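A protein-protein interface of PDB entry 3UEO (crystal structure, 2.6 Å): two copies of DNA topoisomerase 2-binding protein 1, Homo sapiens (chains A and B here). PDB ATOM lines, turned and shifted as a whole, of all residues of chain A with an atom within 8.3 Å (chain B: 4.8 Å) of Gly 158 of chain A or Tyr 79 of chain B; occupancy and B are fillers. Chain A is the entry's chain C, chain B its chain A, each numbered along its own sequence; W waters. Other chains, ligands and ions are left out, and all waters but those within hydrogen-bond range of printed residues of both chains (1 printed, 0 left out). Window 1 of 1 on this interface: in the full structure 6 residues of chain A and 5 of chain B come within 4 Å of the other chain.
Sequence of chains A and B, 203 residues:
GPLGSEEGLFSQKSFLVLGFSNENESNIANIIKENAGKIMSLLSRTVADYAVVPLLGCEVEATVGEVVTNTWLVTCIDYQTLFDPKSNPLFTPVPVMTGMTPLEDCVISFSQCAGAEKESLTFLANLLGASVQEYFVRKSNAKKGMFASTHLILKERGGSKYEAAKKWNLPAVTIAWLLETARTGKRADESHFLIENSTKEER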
ATOM      1  N   SER A 111       4.594 -21.500  -5.844  1.00  0.00           N
ATOM      2  CA  SER A 111       5.948 -21.062  -5.652  1.00  0.00           C
ATOM      3  C   SER A 111       6.019 -19.618  -6.105  1.00  0.00           C
ATOM      4  O   SER A 111       5.316 -19.213  -7.030  1.00  0.00           O
ATOM      5  CB  SER A 111       6.911 -21.949  -6.420  1.00  0.00           C
ATOM      6  OG  SER A 111       8.233 -21.449  -6.331  1.00  0.00           O
ATOM      7  N   GLN A 112       6.826 -18.836  -5.403  1.00  0.00           N
ATOM      8  CA  GLN A 112       7.055 -17.436  -5.730  1.00  0.00           C
ATOM      9  C   GLN A 112       5.847 -16.529  -5.442  1.00  0.00           C
ATOM     10  O   GLN A 112       5.806 -15.369  -5.874  1.00  0.00           O
ATOM     11  CB  GLN A 112       7.562 -17.305  -7.175  1.00  0.00           C
ATOM     12  CG  GLN A 112       8.738 -18.221  -7.460  1.00  0.00           C
ATOM     13  CD  GLN A 112       8.964 -18.473  -8.930  1.00  0.00           C
ATOM     14  OE1 GLN A 112       8.147 -18.104  -9.781  1.00  0.00           O
ATOM     15  NE2 GLN A 112      10.073 -19.124  -9.243  1.00  0.00           N
ATOM     16  N   LEU A 152       2.506 -27.539 -10.238  1.00  0.00           N
ATOM     17  CA  LEU A 152       3.169 -26.417  -9.578  1.00  0.00           C
ATOM     18  C   LEU A 152       2.658 -25.141 -10.235  1.00  0.00           C
ATOM     19  O   LEU A 152       2.589 -25.074 -11.468  1.00  0.00           O
ATOM     20  CB  LEU A 152       4.688 -26.519  -9.709  1.00  0.00           C
ATOM     21  CG  LEU A 152       5.512 -25.440  -8.985  1.00  0.00           C
ATOM     22  CD1 LEU A 152       5.394 -25.524  -7.449  1.00  0.00           C
ATOM     23  CD2 LEU A 152       6.974 -25.471  -9.393  1.00  0.00           C
ATOM     24  N   LEU A 154       3.448 -21.073 -10.529  1.00  0.00           N
ATOM     25  CA  LEU A 154       4.463 -20.051 -10.232  1.00  0.00           C
ATOM     26  C   LEU A 154       4.539 -18.896 -11.224  1.00  0.00           C
ATOM     27  O   LEU A 154       3.662 -18.738 -12.080  1.00  0.00           O
ATOM     28  CB  LEU A 154       5.860 -20.668 -10.110  1.00  0.00           C
ATOM     29  CG  LEU A 154       6.351 -21.746 -11.077  1.00  0.00           C
ATOM     30  CD1 LEU A 154       5.794 -21.586 -12.468  1.00  0.00           C
ATOM     31  CD2 LEU A 154       7.855 -21.759 -11.099  1.00  0.00           C
ATOM     32  N   LYS A 155       5.630 -18.135 -11.125  1.00  0.00           N
ATOM     33  CA  LYS A 155       5.793 -16.875 -11.857  1.00  0.00           C
ATOM     34  C   LYS A 155       6.946 -16.813 -12.856  1.00  0.00           C
ATOM     35  O   LYS A 155       6.727 -16.443 -14.013  1.00  0.00           O
ATOM     36  CB  LYS A 155       5.915 -15.713 -10.885  1.00  0.00           C
ATOM     37  CG  LYS A 155       4.659 -15.495 -10.083  1.00  0.00           C
ATOM     38  CD  LYS A 155       4.663 -14.094  -9.558  1.00  0.00           C
ATOM     39  CE  LYS A 155       3.392 -13.781  -8.840  1.00  0.00           C
ATOM     40  NZ  LYS A 155       3.517 -12.464  -8.163  1.00  0.00           N
ATOM     41  N   GLU A 156       8.163 -17.131 -12.406  1.00  0.00           N
ATOM     42  CA  GLU A 156       9.325 -17.235 -13.288  1.00  0.00           C
ATOM     43  C   GLU A 156       9.853 -18.655 -13.314  1.00  0.00           C
ATOM     44  O   GLU A 156       9.373 -19.516 -12.583  1.00  0.00           O
ATOM     45  CB  GLU A 156      10.463 -16.359 -12.801  1.00  0.00           C
ATOM     46  CG  GLU A 156      10.250 -14.887 -12.872  1.00  0.00           C
ATOM     47  CD  GLU A 156      11.236 -14.190 -11.983  1.00  0.00           C
ATOM     48  OE1 GLU A 156      11.673 -14.821 -10.991  1.00  0.00           O
ATOM     49  OE2 GLU A 156      11.588 -13.033 -12.279  1.00  0.00           O
ATOM     50  N   ARG A 157      10.838 -18.891 -14.174  1.00  0.00           N
ATOM     51  CA  ARG A 157      11.696 -20.057 -14.048  1.00  0.00           C
ATOM     52  C   ARG A 157      12.641 -19.732 -12.937  1.00  0.00           C
ATOM     53  O   ARG A 157      13.249 -18.666 -12.946  1.00  0.00           O
ATOM     54  CB  ARG A 157      12.537 -20.263 -15.295  1.00  0.00           C
ATOM     55  CG  ARG A 157      11.742 -20.462 -16.538  1.00  0.00           C
ATOM     56  CD  ARG A 157      12.648 -20.645 -17.745  1.00  0.00           C
ATOM     57  NE  ARG A 157      11.808 -20.731 -18.913  1.00  0.00           N
ATOM     58  CZ  ARG A 157      11.277 -19.660 -19.490  1.00  0.00           C
ATOM     59  NH1 ARG A 157      11.549 -18.448 -19.017  1.00  0.00           N
ATOM     60  NH2 ARG A 157      10.486 -19.793 -20.548  1.00  0.00           N
ATOM     61  N   GLY A 158      12.788 -20.645 -11.989  1.00  0.00           N
ATOM     62  CA  GLY A 158      13.739 -20.451 -10.911  1.00  0.00           C
ATOM     63  C   GLY A 158      13.320 -21.143  -9.637  1.00  0.00           C
ATOM     64  O   GLY A 158      12.131 -21.419  -9.423  1.00  0.00           O
ATOM     65  N   GLY A 159      14.301 -21.447  -8.795  1.00  0.00           N
ATOM     66  CA  GLY A 159      14.009 -21.950  -7.472  1.00  0.00           C
ATOM     67  C   GLY A 159      13.840 -23.448  -7.414  1.00  0.00           C
ATOM     68  O   GLY A 159      13.648 -24.100  -8.447  1.00  0.00           O
ATOM     69  N   SER A 160      13.886 -23.977  -6.191  1.00  0.00           N
ATOM     70  CA  SER A 160      13.865 -25.418  -5.937  1.00  0.00           C
ATOM     71  C   SER A 160      12.530 -26.083  -6.275  1.00  0.00           C
ATOM     72  O   SER A 160      12.489 -27.255  -6.628  1.00  0.00           O
ATOM     73  CB  SER A 160      14.261 -25.694  -4.481  1.00  0.00           C
ATOM     74  OG  SER A 160      15.177 -24.701  -4.026  1.00  0.00           O
ATOM     75  N   LYS A 161      11.431 -25.350  -6.177  1.00  0.00           N
ATOM     76  CA  LYS A 161      10.150 -25.979  -6.509  1.00  0.00           C
ATOM     77  C   LYS A 161      10.080 -26.250  -7.998  1.00  0.00           C
ATOM     78  O   LYS A 161       9.782 -27.366  -8.411  1.00  0.00           O
ATOM     79  CB  LYS A 161       8.959 -25.170  -6.002  1.00  0.00           C
ATOM     80  CG  LYS A 161       8.573 -25.535  -4.557  1.00  0.00           C
ATOM     81  CD  LYS A 161       7.284 -24.828  -4.132  1.00  0.00           C
ATOM     82  CE  LYS A 161       6.982 -25.032  -2.652  1.00  0.00           C
ATOM     83  NZ  LYS A 161       5.613 -24.519  -2.277  1.00  0.00           N
ATOM     84  N   TYR A 162      10.410 -25.230  -8.793  1.00  0.00           N
ATOM     85  CA  TYR A 162      10.570 -25.356 -10.236  1.00  0.00           C
ATOM     86  C   TYR A 162      11.530 -26.495 -10.660  1.00  0.00           C
ATOM     87  O   TYR A 162      11.250 -27.232 -11.609  1.00  0.00           O
ATOM     88  CB  TYR A 162      11.035 -24.016 -10.802  1.00  0.00           C
ATOM     89  CG  TYR A 162      11.331 -24.051 -12.280  1.00  0.00           C
ATOM     90  CD1 TYR A 162      10.298 -24.117 -13.210  1.00  0.00           C
ATOM     91  CD2 TYR A 162      12.643 -24.015 -12.753  1.00  0.00           C
ATOM     92  CE1 TYR A 162      10.560 -24.157 -14.563  1.00  0.00           C
ATOM     93  CE2 TYR A 162      12.910 -24.054 -14.120  1.00  0.00           C
ATOM     94  CZ  TYR A 162      11.859 -24.126 -15.007  1.00  0.00           C
ATOM     95  OH  TYR A 162      12.089 -24.169 -16.349  1.00  0.00           O
ATOM     96  N   GLU A 163      12.646 -26.660  -9.953  1.00  0.00           N
ATOM     97  CA  GLU A 163      13.640 -27.640 -10.358  1.00  0.00           C
ATOM     98  C   GLU A 163      13.145 -29.040 -10.114  1.00  0.00           C
ATOM     99  O   GLU A 163      13.486 -29.970 -10.848  1.00  0.00           O
ATOM    100  CB  GLU A 163      14.939 -27.428  -9.604  1.00  0.00           C
ATOM    101  CG  GLU A 163      15.689 -26.207 -10.048  1.00  0.00           C
ATOM    102  CD  GLU A 163      16.990 -26.036  -9.297  1.00  0.00           C
ATOM    103  OE1 GLU A 163      17.233 -26.843  -8.356  1.00  0.00           O
ATOM    104  OE2 GLU A 163      17.761 -25.101  -9.657  1.00  0.00           O
ATOM    105  N   ALA A 164      12.359 -29.192  -9.058  1.00  0.00           N
ATOM    106  CA  ALA A 164      11.741 -30.470  -8.747  1.00  0.00           C
ATOM    107  C   ALA A 164      10.686 -30.790  -9.809  1.00  0.00           C
ATOM    108  O   ALA A 164      10.583 -31.928 -10.274  1.00  0.00           O
ATOM    109  CB  ALA A 164      11.112 -30.439  -7.351  1.00  0.00           C
ATOM    110  N   LYS A 166      10.637 -29.905 -12.936  1.00  0.00           N
ATOM    111  CA  LYS A 166      11.274 -30.349 -14.180  1.00  0.00           C
ATOM    112  C   LYS A 166      11.798 -31.766 -14.012  1.00  0.00           C
ATOM    113  O   LYS A 166      11.696 -32.588 -14.903  1.00  0.00           O
ATOM    114  CB  LYS A 166      12.402 -29.415 -14.613  1.00  0.00           C
ATOM    115  CG  LYS A 166      11.991 -27.969 -14.834  1.00  0.00           C
ATOM    116  CD  LYS A 166      11.277 -27.807 -16.157  1.00  0.00           C
ATOM    117  CE  LYS A 166      12.205 -28.112 -17.340  1.00  0.00           C
ATOM    118  NZ  LYS A 166      13.426 -27.264 -17.303  1.00  0.00           N
ATOM    119  N   ILE A 195       5.515 -22.671 -17.633  1.00  0.00           N
ATOM    120  CA  ILE A 195       6.393 -21.553 -17.322  1.00  0.00           C
ATOM    121  C   ILE A 195       7.648 -21.698 -18.184  1.00  0.00           C
ATOM    122  O   ILE A 195       8.327 -20.712 -18.492  1.00  0.00           O
ATOM    123  CB  ILE A 195       6.750 -21.536 -15.831  1.00  0.00           C
ATOM    124  CG1 ILE A 195       7.533 -20.280 -15.481  1.00  0.00           C
ATOM    125  CG2 ILE A 195       7.564 -22.737 -15.477  1.00  0.00           C
ATOM    126  CD1 ILE A 195       6.772 -19.021 -15.745  1.00  0.00           C
ATOM    127  N   GLU A 196       7.902 -22.942 -18.598  1.00  0.00           N
ATOM    128  CA  GLU A 196       8.992 -23.309 -19.480  1.00  0.00           C
ATOM    129  C   GLU A 196       8.971 -22.538 -20.780  1.00  0.00           C
ATOM    130  O   GLU A 196      10.006 -22.367 -21.420  1.00  0.00           O
ATOM    131  CB  GLU A 196       8.903 -24.789 -19.820  1.00  0.00           C
ATOM    132  CG  GLU A 196      10.158 -25.330 -20.435  1.00  0.00           C
ATOM    133  CD  GLU A 196      11.327 -25.279 -19.467  1.00  0.00           C
ATOM    134  OE1 GLU A 196      11.077 -25.338 -18.245  1.00  0.00           O
ATOM    135  OE2 GLU A 196      12.488 -25.174 -19.924  1.00  0.00           O
ATOM    136  N   SER A 198       7.050 -19.505 -21.067  1.00  0.00           N
ATOM    137  CA  SER A 198       6.680 -18.119 -20.793  1.00  0.00           C
ATOM    138  C   SER A 198       7.787 -17.127 -21.169  1.00  0.00           C
ATOM    139  O   SER A 198       8.969 -17.370 -20.911  1.00  0.00           O
ATOM    140  CB  SER A 198       6.305 -17.949 -19.314  1.00  0.00           C
ATOM    141  OG  SER A 198       5.820 -16.638 -19.059  1.00  0.00           O
ATOM    142  N   THR B  75      23.356 -21.444 -14.948  1.00  0.00           N
ATOM    143  CA  THR B  75      22.236 -20.721 -14.395  1.00  0.00           C
ATOM    144  C   THR B  75      21.432 -20.115 -15.530  1.00  0.00           C
ATOM    145  O   THR B  75      20.226 -20.308 -15.611  1.00  0.00           O
ATOM    146  CB  THR B  75      22.732 -19.624 -13.448  1.00  0.00           C
ATOM    147  OG1 THR B  75      23.264 -20.233 -12.265  1.00  0.00           O
ATOM    148  CG2 THR B  75      21.610 -18.704 -13.055  1.00  0.00           C
ATOM    149  N   CYS B  76      22.119 -19.407 -16.423  1.00  0.00           N
ATOM    150  CA  CYS B  76      21.480 -18.745 -17.564  1.00  0.00           C
ATOM    151  C   CYS B  76      20.608 -19.716 -18.336  1.00  0.00           C
ATOM    152  O   CYS B  76      19.466 -19.433 -18.670  1.00  0.00           O
ATOM    153  CB  CYS B  76      22.527 -18.144 -18.491  1.00  0.00           C
ATOM    154  SG  CYS B  76      22.857 -16.411 -18.143  1.00  0.00           S
ATOM    155  N   ILE B  77      21.163 -20.884 -18.588  1.00  0.00           N
ATOM    156  CA  ILE B  77      20.451 -21.921 -19.281  1.00  0.00           C
ATOM    157  C   ILE B  77      19.311 -22.483 -18.452  1.00  0.00           C
ATOM    158  O   ILE B  77      18.180 -22.521 -18.911  1.00  0.00           O
ATOM    159  CB  ILE B  77      21.437 -22.995 -19.656  1.00  0.00           C
ATOM    160  CG1 ILE B  77      22.384 -22.388 -20.687  1.00  0.00           C
ATOM    161  CG2 ILE B  77      20.723 -24.242 -20.162  1.00  0.00           C
ATOM    162  CD1 ILE B  77      23.536 -23.224 -21.018  1.00  0.00           C
ATOM    163  N   ASP B  78      19.602 -22.900 -17.226  1.00  0.00           N
ATOM    164  CA  ASP B  78      18.566 -23.419 -16.331  1.00  0.00           C
ATOM    165  C   ASP B  78      17.312 -22.531 -16.232  1.00  0.00           C
ATOM    166  O   ASP B  78      16.193 -23.033 -16.115  1.00  0.00           O
ATOM    167  CB  ASP B  78      19.144 -23.698 -14.940  1.00  0.00           C
ATOM    168  CG  ASP B  78      19.988 -24.976 -14.900  1.00  0.00           C
ATOM    169  OD1 ASP B  78      19.864 -25.789 -15.848  1.00  0.00           O
ATOM    170  OD2 ASP B  78      20.762 -25.179 -13.924  1.00  0.00           O
ATOM    171  N   TYR B  79      17.494 -21.217 -16.298  1.00  0.00           N
ATOM    172  CA  TYR B  79      16.380 -20.294 -16.115  1.00  0.00           C
ATOM    173  C   TYR B  79      15.980 -19.599 -17.417  1.00  0.00           C
ATOM    174  O   TYR B  79      15.174 -18.659 -17.405  1.00  0.00           O
ATOM    175  CB  TYR B  79      16.709 -19.282 -15.013  1.00  0.00           C
ATOM    176  CG  TYR B  79      16.900 -19.943 -13.660  1.00  0.00           C
ATOM    177  CD1 TYR B  79      16.415 -21.233 -13.423  1.00  0.00           C
ATOM    178  CD2 TYR B  79      17.563 -19.289 -12.620  1.00  0.00           C
ATOM    179  CE1 TYR B  79      16.589 -21.861 -12.201  1.00  0.00           C
ATOM    180  CE2 TYR B  79      17.740 -19.909 -11.384  1.00  0.00           C
ATOM    181  CZ  TYR B  79      17.247 -21.198 -11.179  1.00  0.00           C
ATOM    182  OH  TYR B  79      17.403 -21.831  -9.956  1.00  0.00           O
ATOM    183  N   GLN B  80      16.535 -20.099 -18.527  1.00  0.00           N
ATOM    184  CA  GLN B  80      16.377 -19.533 -19.876  1.00  0.00           C
ATOM    185  C   GLN B  80      16.374 -18.017 -19.874  1.00  0.00           C
ATOM    186  O   GLN B  80      15.580 -17.392 -20.573  1.00  0.00           O
ATOM    187  CB  GLN B  80      15.119 -20.068 -20.570  1.00  0.00           C
ATOM    188  CG  GLN B  80      15.061 -21.592 -20.692  1.00  0.00           C
ATOM    189  CD  GLN B  80      16.049 -22.158 -21.712  1.00  0.00           C
ATOM    190  OE1 GLN B  80      16.758 -21.414 -22.400  1.00  0.00           O
ATOM    191  NE2 GLN B  80      16.089 -23.488 -21.816  1.00  0.00           N
ATOM    192  N   THR B  81      17.267 -17.441 -19.078  1.00  0.00           N
ATOM    193  CA  THR B  81      17.402 -15.997 -18.941  1.00  0.00           C
ATOM    194  C   THR B  81      18.866 -15.577 -19.063  1.00  0.00           C
ATOM    195  O   THR B  81      19.745 -16.210 -18.498  1.00  0.00           O
ATOM    196  CB  THR B  81      16.872 -15.534 -17.582  1.00  0.00           C
ATOM    197  OG1 THR B  81      15.540 -16.033 -17.399  1.00  0.00           O
ATOM    198  CG2 THR B  81      16.867 -14.014 -17.499  1.00  0.00           C
ATOM    199  N   PHE B  83      21.087 -13.549 -17.719  1.00  0.00           N
ATOM    200  CA  PHE B  83      21.379 -12.715 -16.557  1.00  0.00           C
ATOM    201  C   PHE B  83      22.594 -11.874 -16.840  1.00  0.00           C
ATOM    202  O   PHE B  83      23.535 -12.354 -17.447  1.00  0.00           O
ATOM    203  CB  PHE B  83      21.651 -13.576 -15.325  1.00  0.00           C
ATOM    204  CG  PHE B  83      20.492 -14.438 -14.914  1.00  0.00           C
ATOM    205  CD1 PHE B  83      19.379 -13.885 -14.289  1.00  0.00           C
ATOM    206  CD2 PHE B  83      20.513 -15.801 -15.144  1.00  0.00           C
ATOM    207  CE1 PHE B  83      18.304 -14.680 -13.908  1.00  0.00           C
ATOM    208  CE2 PHE B  83      19.435 -16.605 -14.762  1.00  0.00           C
ATOM    209  CZ  PHE B  83      18.328 -16.038 -14.147  1.00  0.00           C
ATOM    210  N   ALA B 114      19.513 -22.389  -4.847  1.00  0.00           N
ATOM    211  CA  ALA B 114      19.095 -23.533  -5.640  1.00  0.00           C
ATOM    212  C   ALA B 114      20.053 -23.844  -6.773  1.00  0.00           C
ATOM    213  O   ALA B 114      20.633 -22.945  -7.356  1.00  0.00           O
ATOM    214  CB  ALA B 114      17.696 -23.295  -6.184  1.00  0.00           C
HETATM  215  O   HOH W   1      13.699 -16.239 -15.281  1.00  0.00           O
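N of Gly 159 of chain A sits at hydrogen-bond distance from OH of Tyr 79 of chain B (3.3 Å). OE2 of Glu 163 of chain A sits at hydrogen-bond distance from OH of Tyr 79 of chain B.
The backbone carbonyl oxygen of Tyr 79 of chain B sits at hydrogen-bond distance from the side-chain hydroxyl of Thr 81 of chain B (2.7 Å). NE2 of Gln 112 of chain A sits at hydrogen-bond distance from O of Gly 158 of chain A (3.1 Å). The guanidinium group of Arg 157 of chain A is in hydrogen-bond range of the backbone carbonyl oxygen of Ile 195 of chain A, at 3.1 Å. The guanidinium group (NH2) of Arg 157 of chain A sits at hydrogen-bond distance from the backbone carbonyl oxygen (O) of Glu 196 of chain A (2.8 Å). The guanidinium group of Arg 157 of chain A is in hydrogen-bond range of the backbone carbonyl oxygen of Ser 198 of chain A (2.9 Å). The side-chain hydroxyl of Tyr 162 of chain A is in hydrogen-bond range of the side-chain carboxylate of Glu 196 of chain A, 2.4 Å away.
Arg 157 of chain A touches Tyr 79 of chain B (CD to O, 3.2 Å). Arg 157 of chain A touches Gln 80 of chain B. Tyr 79 of chain B touches Gly 158 of chain A (CE1 to CA, 3.4 Å). Ser 160 of chain A touches Ala 114 of chain B. Tyr 162 of chain A touches Asp 78 of chain B (CE2 to O, 3.97 Å). OE2 of Glu 163 of chain A touches C of Ala 114 of chain B (3.9 Å).
Of chain B, only Tyr 79 (3.4 Å) comes within 4 Å of Gly 158 of chain A. Tyr 79 of chain B touches just these residues of chain A: Arg 157 (3.2 Å), Gly 158 (3.4 Å), Gly 159 (3.3 Å) and Glu 163 (3.3 Å). Of the printed residues of chain B, Arg 157 of chain A touches Tyr 79 (3.2 Å) and Gln 80 (3.8 Å). Printed residues of chain B within 4 Å of Tyr 162 of chain A: Asp 78. Of the printed residues of chain A, Asp 78 of chain B touches Tyr 162. Of the printed residues of chain A, Ala 114 of chain B touches Ser 160 (3.6 Å) and Glu 163 (3.9 Å). Glu 196 of chain A touches none of the printed residues of chain B. The nearest residue of chain A that does not touch Tyr 79 of chain B is Tyr 162 of chain A (4.5 Å). The nearest printed residue of chain B that does not touch Glu 163 of chain A is Asp 78 of chain B (5.2 Å).
Of the 9 printed residues of chain B, 4 touch a printed residue of chain A. Hydrophobic or aromatic side chains of chain A that line the printed part of chain B: Tyr 162.
No position is printed for both chains. Of the 8 pairs that touch across the chains among the printed residues, none has its exchanged pair printed and touching as well.
Water W1 bridges OG1 of Thr 81 of chain B (2.8 Å) and O of Arg 157 of chain A (3.4 Å).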
